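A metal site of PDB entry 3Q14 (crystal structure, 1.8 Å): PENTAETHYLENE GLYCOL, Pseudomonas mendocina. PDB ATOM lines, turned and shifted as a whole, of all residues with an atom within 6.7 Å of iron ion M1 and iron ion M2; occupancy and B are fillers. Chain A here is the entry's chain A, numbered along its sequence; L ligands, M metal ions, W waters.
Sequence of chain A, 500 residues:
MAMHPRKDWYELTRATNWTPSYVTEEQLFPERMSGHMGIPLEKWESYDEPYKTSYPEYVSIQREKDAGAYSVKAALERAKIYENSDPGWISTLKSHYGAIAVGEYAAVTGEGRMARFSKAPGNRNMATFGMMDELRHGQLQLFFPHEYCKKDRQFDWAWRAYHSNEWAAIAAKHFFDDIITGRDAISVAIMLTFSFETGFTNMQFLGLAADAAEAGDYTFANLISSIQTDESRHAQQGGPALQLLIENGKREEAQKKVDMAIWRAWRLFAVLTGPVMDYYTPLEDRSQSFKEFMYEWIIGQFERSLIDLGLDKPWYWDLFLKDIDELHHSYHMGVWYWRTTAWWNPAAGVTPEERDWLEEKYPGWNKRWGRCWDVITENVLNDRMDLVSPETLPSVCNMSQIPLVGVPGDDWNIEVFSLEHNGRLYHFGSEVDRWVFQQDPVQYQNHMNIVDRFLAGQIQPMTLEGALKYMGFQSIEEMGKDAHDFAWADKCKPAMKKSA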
ATOM      1  N   GLU A 104      20.915  26.401  15.722  1.00  0.00           N
ATOM      2  CA  GLU A 104      21.934  25.906  14.791  1.00  0.00           C
ATOM      3  C   GLU A 104      21.706  26.527  13.428  1.00  0.00           C
ATOM      4  O   GLU A 104      22.633  26.961  12.763  1.00  0.00           O
ATOM      5  CB  GLU A 104      21.860  24.378  14.650  1.00  0.00           C
ATOM      6  CG  GLU A 104      22.130  23.641  15.942  1.00  0.00           C
ATOM      7  CD  GLU A 104      23.578  23.243  16.096  1.00  0.00           C
ATOM      8  OE1 GLU A 104      23.841  22.289  16.850  1.00  0.00           O
ATOM      9  OE2 GLU A 104      24.443  23.888  15.466  1.00  0.00           O
ATOM     10  N   ALA A 107      22.931  29.889  13.277  1.00  0.00           N
ATOM     11  CA  ALA A 107      24.383  29.978  13.192  1.00  0.00           C
ATOM     12  C   ALA A 107      24.870  29.952  11.745  1.00  0.00           C
ATOM     13  O   ALA A 107      25.989  30.378  11.461  1.00  0.00           O
ATOM     14  CB  ALA A 107      25.045  28.847  13.994  1.00  0.00           C
ATOM     15  N   GLU A 111      27.999  32.303  10.272  1.00  0.00           N
ATOM     16  CA  GLU A 111      29.045  31.828   9.368  1.00  0.00           C
ATOM     17  C   GLU A 111      28.975  32.591   8.049  1.00  0.00           C
ATOM     18  O   GLU A 111      30.004  32.977   7.498  1.00  0.00           O
ATOM     19  CB  GLU A 111      28.945  30.320   9.156  1.00  0.00           C
ATOM     20  CG  GLU A 111      29.251  29.494  10.404  1.00  0.00           C
ATOM     21  CD  GLU A 111      30.756  29.436  10.741  1.00  0.00           C
ATOM     22  OE1 GLU A 111      31.578  29.830   9.903  1.00  0.00           O
ATOM     23  OE2 GLU A 111      31.100  28.983  11.852  1.00  0.00           O
ATOM     24  N   GLY A 130      31.701  26.200   7.432  1.00  0.00           N
ATOM     25  CA  GLY A 130      30.929  26.471   8.628  1.00  0.00           C
ATOM     26  C   GLY A 130      29.443  26.652   8.343  1.00  0.00           C
ATOM     27  O   GLY A 130      28.597  26.156   9.099  1.00  0.00           O
ATOM     28  N   ASP A 133      28.194  23.193   7.773  1.00  0.00           N
ATOM     29  CA  ASP A 133      28.112  22.441   9.015  1.00  0.00           C
ATOM     30  C   ASP A 133      26.847  22.817   9.808  1.00  0.00           C
ATOM     31  O   ASP A 133      26.182  21.961  10.357  1.00  0.00           O
ATOM     32  CB  ASP A 133      29.303  22.728   9.935  1.00  0.00           C
ATOM     33  CG  ASP A 133      30.624  22.214   9.401  1.00  0.00           C
ATOM     34  OD1 ASP A 133      30.641  21.277   8.574  1.00  0.00           O
ATOM     35  OD2 ASP A 133      31.661  22.742   9.876  1.00  0.00           O
ATOM     36  N   GLU A 134      26.565  24.103   9.935  1.00  0.00           N
ATOM     37  CA  GLU A 134      25.427  24.506  10.751  1.00  0.00           C
ATOM     38  C   GLU A 134      24.117  24.120  10.067  1.00  0.00           C
ATOM     39  O   GLU A 134      23.126  23.825  10.724  1.00  0.00           O
ATOM     40  CB  GLU A 134      25.446  26.002  11.094  1.00  0.00           C
ATOM     41  CG  GLU A 134      26.721  26.494  11.838  1.00  0.00           C
ATOM     42  CD  GLU A 134      26.967  25.799  13.187  1.00  0.00           C
ATOM     43  OE1 GLU A 134      26.257  24.850  13.572  1.00  0.00           O
ATOM     44  OE2 GLU A 134      27.876  26.265  13.895  1.00  0.00           O
ATOM     45  N   HIS A 137      23.633  20.675  11.086  1.00  0.00           N
ATOM     46  CA  HIS A 137      23.214  20.554  12.473  1.00  0.00           C
ATOM     47  C   HIS A 137      21.766  20.916  12.673  1.00  0.00           C
ATOM     48  O   HIS A 137      21.069  20.253  13.418  1.00  0.00           O
ATOM     49  CB  HIS A 137      24.085  21.404  13.372  1.00  0.00           C
ATOM     50  CG  HIS A 137      25.535  21.046  13.284  1.00  0.00           C
ATOM     51  ND1 HIS A 137      26.522  21.808  13.860  1.00  0.00           N
ATOM     52  CD2 HIS A 137      26.158  19.999  12.690  1.00  0.00           C
ATOM     53  CE1 HIS A 137      27.697  21.251  13.623  1.00  0.00           C
ATOM     54  NE2 HIS A 137      27.505  20.152  12.904  1.00  0.00           N
ATOM     55  N   GLY A 138      21.315  21.955  11.982  1.00  0.00           N
ATOM     56  CA  GLY A 138      19.922  22.363  12.072  1.00  0.00           C
ATOM     57  C   GLY A 138      19.039  21.277  11.502  1.00  0.00           C
ATOM     58  O   GLY A 138      17.994  20.936  12.070  1.00  0.00           O
ATOM     59  N   GLN A 141      18.877  18.131  13.720  1.00  0.00           N
ATOM     60  CA  GLN A 141      18.189  18.295  14.984  1.00  0.00           C
ATOM     61  C   GLN A 141      16.727  18.694  14.847  1.00  0.00           C
ATOM     62  O   GLN A 141      16.023  18.824  15.830  1.00  0.00           O
ATOM     63  CB  GLN A 141      19.000  19.217  15.913  1.00  0.00           C
ATOM     64  CG  GLN A 141      20.259  18.487  16.390  1.00  0.00           C
ATOM     65  CD  GLN A 141      21.236  19.395  17.091  1.00  0.00           C
ATOM     66  OE1 GLN A 141      21.765  20.332  16.491  1.00  0.00           O
ATOM     67  NE2 GLN A 141      21.481  19.113  18.356  1.00  0.00           N
ATOM     68  N   LEU A 192      31.200  33.846  18.739  1.00  0.00           N
ATOM     69  CA  LEU A 192      30.626  32.569  18.388  1.00  0.00           C
ATOM     70  C   LEU A 192      31.706  31.492  18.259  1.00  0.00           C
ATOM     71  O   LEU A 192      31.730  30.541  19.022  1.00  0.00           O
ATOM     72  CB  LEU A 192      29.824  32.667  17.093  1.00  0.00           C
ATOM     73  CG  LEU A 192      29.336  31.317  16.533  1.00  0.00           C
ATOM     74  CD1 LEU A 192      28.412  30.615  17.512  1.00  0.00           C
ATOM     75  CD2 LEU A 192      28.636  31.574  15.210  1.00  0.00           C
ATOM     76  N   PHE A 196      31.892  30.787  22.369  1.00  0.00           N
ATOM     77  CA  PHE A 196      30.800  29.836  22.507  1.00  0.00           C
ATOM     78  C   PHE A 196      31.199  28.430  22.039  1.00  0.00           C
ATOM     79  O   PHE A 196      30.978  27.436  22.752  1.00  0.00           O
ATOM     80  CB  PHE A 196      29.571  30.340  21.747  1.00  0.00           C
ATOM     81  CG  PHE A 196      28.349  29.474  21.915  1.00  0.00           C
ATOM     82  CD1 PHE A 196      27.748  29.335  23.150  1.00  0.00           C
ATOM     83  CD2 PHE A 196      27.790  28.843  20.820  1.00  0.00           C
ATOM     84  CE1 PHE A 196      26.609  28.544  23.293  1.00  0.00           C
ATOM     85  CE2 PHE A 196      26.647  28.049  20.972  1.00  0.00           C
ATOM     86  CZ  PHE A 196      26.062  27.913  22.203  1.00  0.00           C
ATOM     87  N   GLU A 197      31.800  28.347  20.852  1.00  0.00           N
ATOM     88  CA  GLU A 197      31.983  27.033  20.205  1.00  0.00           C
ATOM     89  C   GLU A 197      33.238  26.276  20.640  1.00  0.00           C
ATOM     90  O   GLU A 197      33.287  25.058  20.498  1.00  0.00           O
ATOM     91  CB  GLU A 197      31.940  27.137  18.681  1.00  0.00           C
ATOM     92  CG  GLU A 197      30.599  27.624  18.128  1.00  0.00           C
ATOM     93  CD  GLU A 197      30.587  27.719  16.602  1.00  0.00           C
ATOM     94  OE1 GLU A 197      31.596  28.168  16.016  1.00  0.00           O
ATOM     95  OE2 GLU A 197      29.578  27.339  16.001  1.00  0.00           O
ATOM     96  N   THR A 201      29.958  24.830  24.074  1.00  0.00           N
ATOM     97  CA  THR A 201      29.120  23.805  23.460  1.00  0.00           C
ATOM     98  C   THR A 201      29.530  22.393  23.834  1.00  0.00           C
ATOM     99  O   THR A 201      28.705  21.480  23.831  1.00  0.00           O
ATOM    100  CB  THR A 201      29.028  23.916  21.941  1.00  0.00           C
ATOM    101  OG1 THR A 201      30.344  23.881  21.384  1.00  0.00           O
ATOM    102  CG2 THR A 201      28.335  25.211  21.527  1.00  0.00           C
ATOM    103  N   PHE A 205      27.034  19.134  24.071  1.00  0.00           N
ATOM    104  CA  PHE A 205      27.130  18.129  23.012  1.00  0.00           C
ATOM    105  C   PHE A 205      28.040  16.932  23.348  1.00  0.00           C
ATOM    106  O   PHE A 205      27.973  15.891  22.670  1.00  0.00           O
ATOM    107  CB  PHE A 205      27.585  18.776  21.706  1.00  0.00           C
ATOM    108  CG  PHE A 205      26.531  19.658  21.095  1.00  0.00           C
ATOM    109  CD1 PHE A 205      26.340  20.963  21.549  1.00  0.00           C
ATOM    110  CD2 PHE A 205      25.721  19.169  20.098  1.00  0.00           C
ATOM    111  CE1 PHE A 205      25.363  21.757  20.986  1.00  0.00           C
ATOM    112  CE2 PHE A 205      24.732  19.966  19.544  1.00  0.00           C
ATOM    113  CZ  PHE A 205      24.563  21.263  19.981  1.00  0.00           C
ATOM    114  N   ILE A 227      27.891  15.696  15.710  1.00  0.00           N
ATOM    115  CA  ILE A 227      27.765  17.122  15.503  1.00  0.00           C
ATOM    116  C   ILE A 227      29.014  17.853  16.016  1.00  0.00           C
ATOM    117  O   ILE A 227      29.538  18.744  15.356  1.00  0.00           O
ATOM    118  CB  ILE A 227      26.468  17.652  16.150  1.00  0.00           C
ATOM    119  CG1 ILE A 227      25.290  17.264  15.262  1.00  0.00           C
ATOM    120  CG2 ILE A 227      26.514  19.171  16.344  1.00  0.00           C
ATOM    121  CD1 ILE A 227      23.909  17.486  15.925  1.00  0.00           C
ATOM    122  N   GLN A 228      29.500  17.450  17.184  1.00  0.00           N
ATOM    123  CA  GLN A 228      30.615  18.176  17.766  1.00  0.00           C
ATOM    124  C   GLN A 228      31.903  17.994  16.968  1.00  0.00           C
ATOM    125  O   GLN A 228      32.801  18.835  17.046  1.00  0.00           O
ATOM    126  CB  GLN A 228      30.824  17.811  19.247  1.00  0.00           C
ATOM    127  CG  GLN A 228      31.511  18.896  20.064  1.00  0.00           C
ATOM    128  CD  GLN A 228      30.671  20.174  20.218  1.00  0.00           C
ATOM    129  OE1 GLN A 228      29.625  20.345  19.590  1.00  0.00           O
ATOM    130  NE2 GLN A 228      31.141  21.076  21.067  1.00  0.00           N
ATOM    131  N   ASP A 230      32.164  18.442  13.876  1.00  0.00           N
ATOM    132  CA  ASP A 230      32.173  19.572  12.953  1.00  0.00           C
ATOM    133  C   ASP A 230      32.527  20.857  13.687  1.00  0.00           C
ATOM    134  O   ASP A 230      33.282  21.701  13.180  1.00  0.00           O
ATOM    135  CB  ASP A 230      30.785  19.811  12.336  1.00  0.00           C
ATOM    136  CG  ASP A 230      30.298  18.663  11.501  1.00  0.00           C
ATOM    137  OD1 ASP A 230      31.124  18.016  10.808  1.00  0.00           O
ATOM    138  OD2 ASP A 230      29.071  18.408  11.516  1.00  0.00           O
ATOM    139  N   GLU A 231      31.935  21.010  14.863  1.00  0.00           N
ATOM    140  CA  GLU A 231      32.185  22.166  15.720  1.00  0.00           C
ATOM    141  C   GLU A 231      33.683  22.294  15.939  1.00  0.00           C
ATOM    142  O   GLU A 231      34.247  23.386  15.871  1.00  0.00           O
ATOM    143  CB  GLU A 231      31.483  21.959  17.064  1.00  0.00           C
ATOM    144  CG  GLU A 231      31.653  23.120  18.047  1.00  0.00           C
ATOM    145  CD  GLU A 231      30.599  24.188  17.841  1.00  0.00           C
ATOM    146  OE1 GLU A 231      29.835  24.488  18.782  1.00  0.00           O
ATOM    147  OE2 GLU A 231      30.528  24.723  16.724  1.00  0.00           O
ATOM    148  N   HIS A 234      35.165  24.002  12.677  1.00  0.00           N
ATOM    149  CA  HIS A 234      34.849  25.393  12.355  1.00  0.00           C
ATOM    150  C   HIS A 234      35.034  26.369  13.514  1.00  0.00           C
ATOM    151  O   HIS A 234      35.213  27.561  13.292  1.00  0.00           O
ATOM    152  CB  HIS A 234      33.480  25.564  11.660  1.00  0.00           C
ATOM    153  CG  HIS A 234      32.292  25.243  12.511  1.00  0.00           C
ATOM    154  ND1 HIS A 234      31.371  24.284  12.138  1.00  0.00           N
ATOM    155  CD2 HIS A 234      31.815  25.794  13.642  1.00  0.00           C
ATOM    156  CE1 HIS A 234      30.401  24.232  13.024  1.00  0.00           C
ATOM    157  NE2 HIS A 234      30.641  25.143  13.954  1.00  0.00           N
ATOM    158  N   ALA A 235      35.049  25.847  14.734  1.00  0.00           N
ATOM    159  CA  ALA A 235      35.312  26.701  15.900  1.00  0.00           C
ATOM    160  C   ALA A 235      36.733  27.248  15.841  1.00  0.00           C
ATOM    161  O   ALA A 235      37.050  28.274  16.467  1.00  0.00           O
ATOM    162  CB  ALA A 235      35.084  25.933  17.225  1.00  0.00           C
HETATM  163  C1  LIG L   1      22.502  26.992  18.966  1.00  0.00           C
HETATM  164  C2  LIG L   1      23.851  26.561  18.466  1.00  0.00           C
HETATM  165  C3  LIG L   1      24.489  27.300  17.477  1.00  0.00           C
HETATM  166  C4  LIG L   1      25.731  26.905  17.012  1.00  0.00           C
HETATM  167  C5  LIG L   1      24.456  25.445  19.007  1.00  0.00           C
HETATM  168  C6  LIG L   1      25.700  25.036  18.540  1.00  0.00           C
HETATM  169  C7  LIG L   1      26.332  25.769  17.546  1.00  0.00           C
HETATM  170  O1  LIG L   1      27.571  25.371  17.091  1.00  0.00           O
HETATM  171 FE    FE M   1      26.436  23.479  15.184  1.00  0.00          FE
HETATM  172 FE    FE M   2      29.062  25.423  15.441  1.00  0.00          FE
HETATM  173  O   HOH W   1      28.519  23.488  15.340  1.00  0.00           O
HETATM  174  O   HOH W   2      26.425  22.246  16.917  1.00  0.00           O
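Within 4 Å of iron ion M2: Glu 134, Glu 197, Glu 231 and His 234.
Iron ion M2 is bound by water W1 (2.0 Å), OE2 of Glu 197 (2.1 Å), OE2 of Glu 231 (2.1 Å), OE2 of Glu 134 (2.1 Å), NE2 of His 234 (2.2 Å) and O1 of the ligand (2.2 Å).
OE2 of Glu 104 binds iron ion M1 (2.1 Å). Iron ion M1 is bound by water W1 (2.1 Å). OE1 of Glu 134 is bound to iron ion M1, at 2.1 Å. Water W2 binds iron ion M1, at 2.1 Å. A ring nitrogen (ND1) of His 137 is bound to iron ion M1, 2.1 Å away.
The side-chain amide oxygen of Gln 141 lies close to the side-chain carboxylate of Glu 104, 2.9 Å away. O of Glu 197 is in hydrogen-bond range of OG1 of Thr 201. The side-chain hydroxyl (OG1) of Thr 201 sits at hydrogen-bond distance from the side-chain carboxylate (OE1) of Glu 231, at 2.7 Å. A ring nitrogen (NE2) of His 137 sits at hydrogen-bond distance from the backbone carbonyl oxygen (O) of Ile 227, at 3.5 Å. A ring nitrogen (NE2) of His 137 lies close to the backbone carbonyl oxygen of Asp 133. OE1 of Gln 141 sits close to O of His 137 (3.2 Å). A ring nitrogen (ND1) of His 234 lies within hydrogen-bond range of the side-chain carboxylate of Asp 133. ND1 of His 234 is in hydrogen-bond range of O of Asp 230, 3.4 Å away.
Three residues have an atom within 4 Å of iron ion M1: Glu 104, Glu 134 and His 137.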
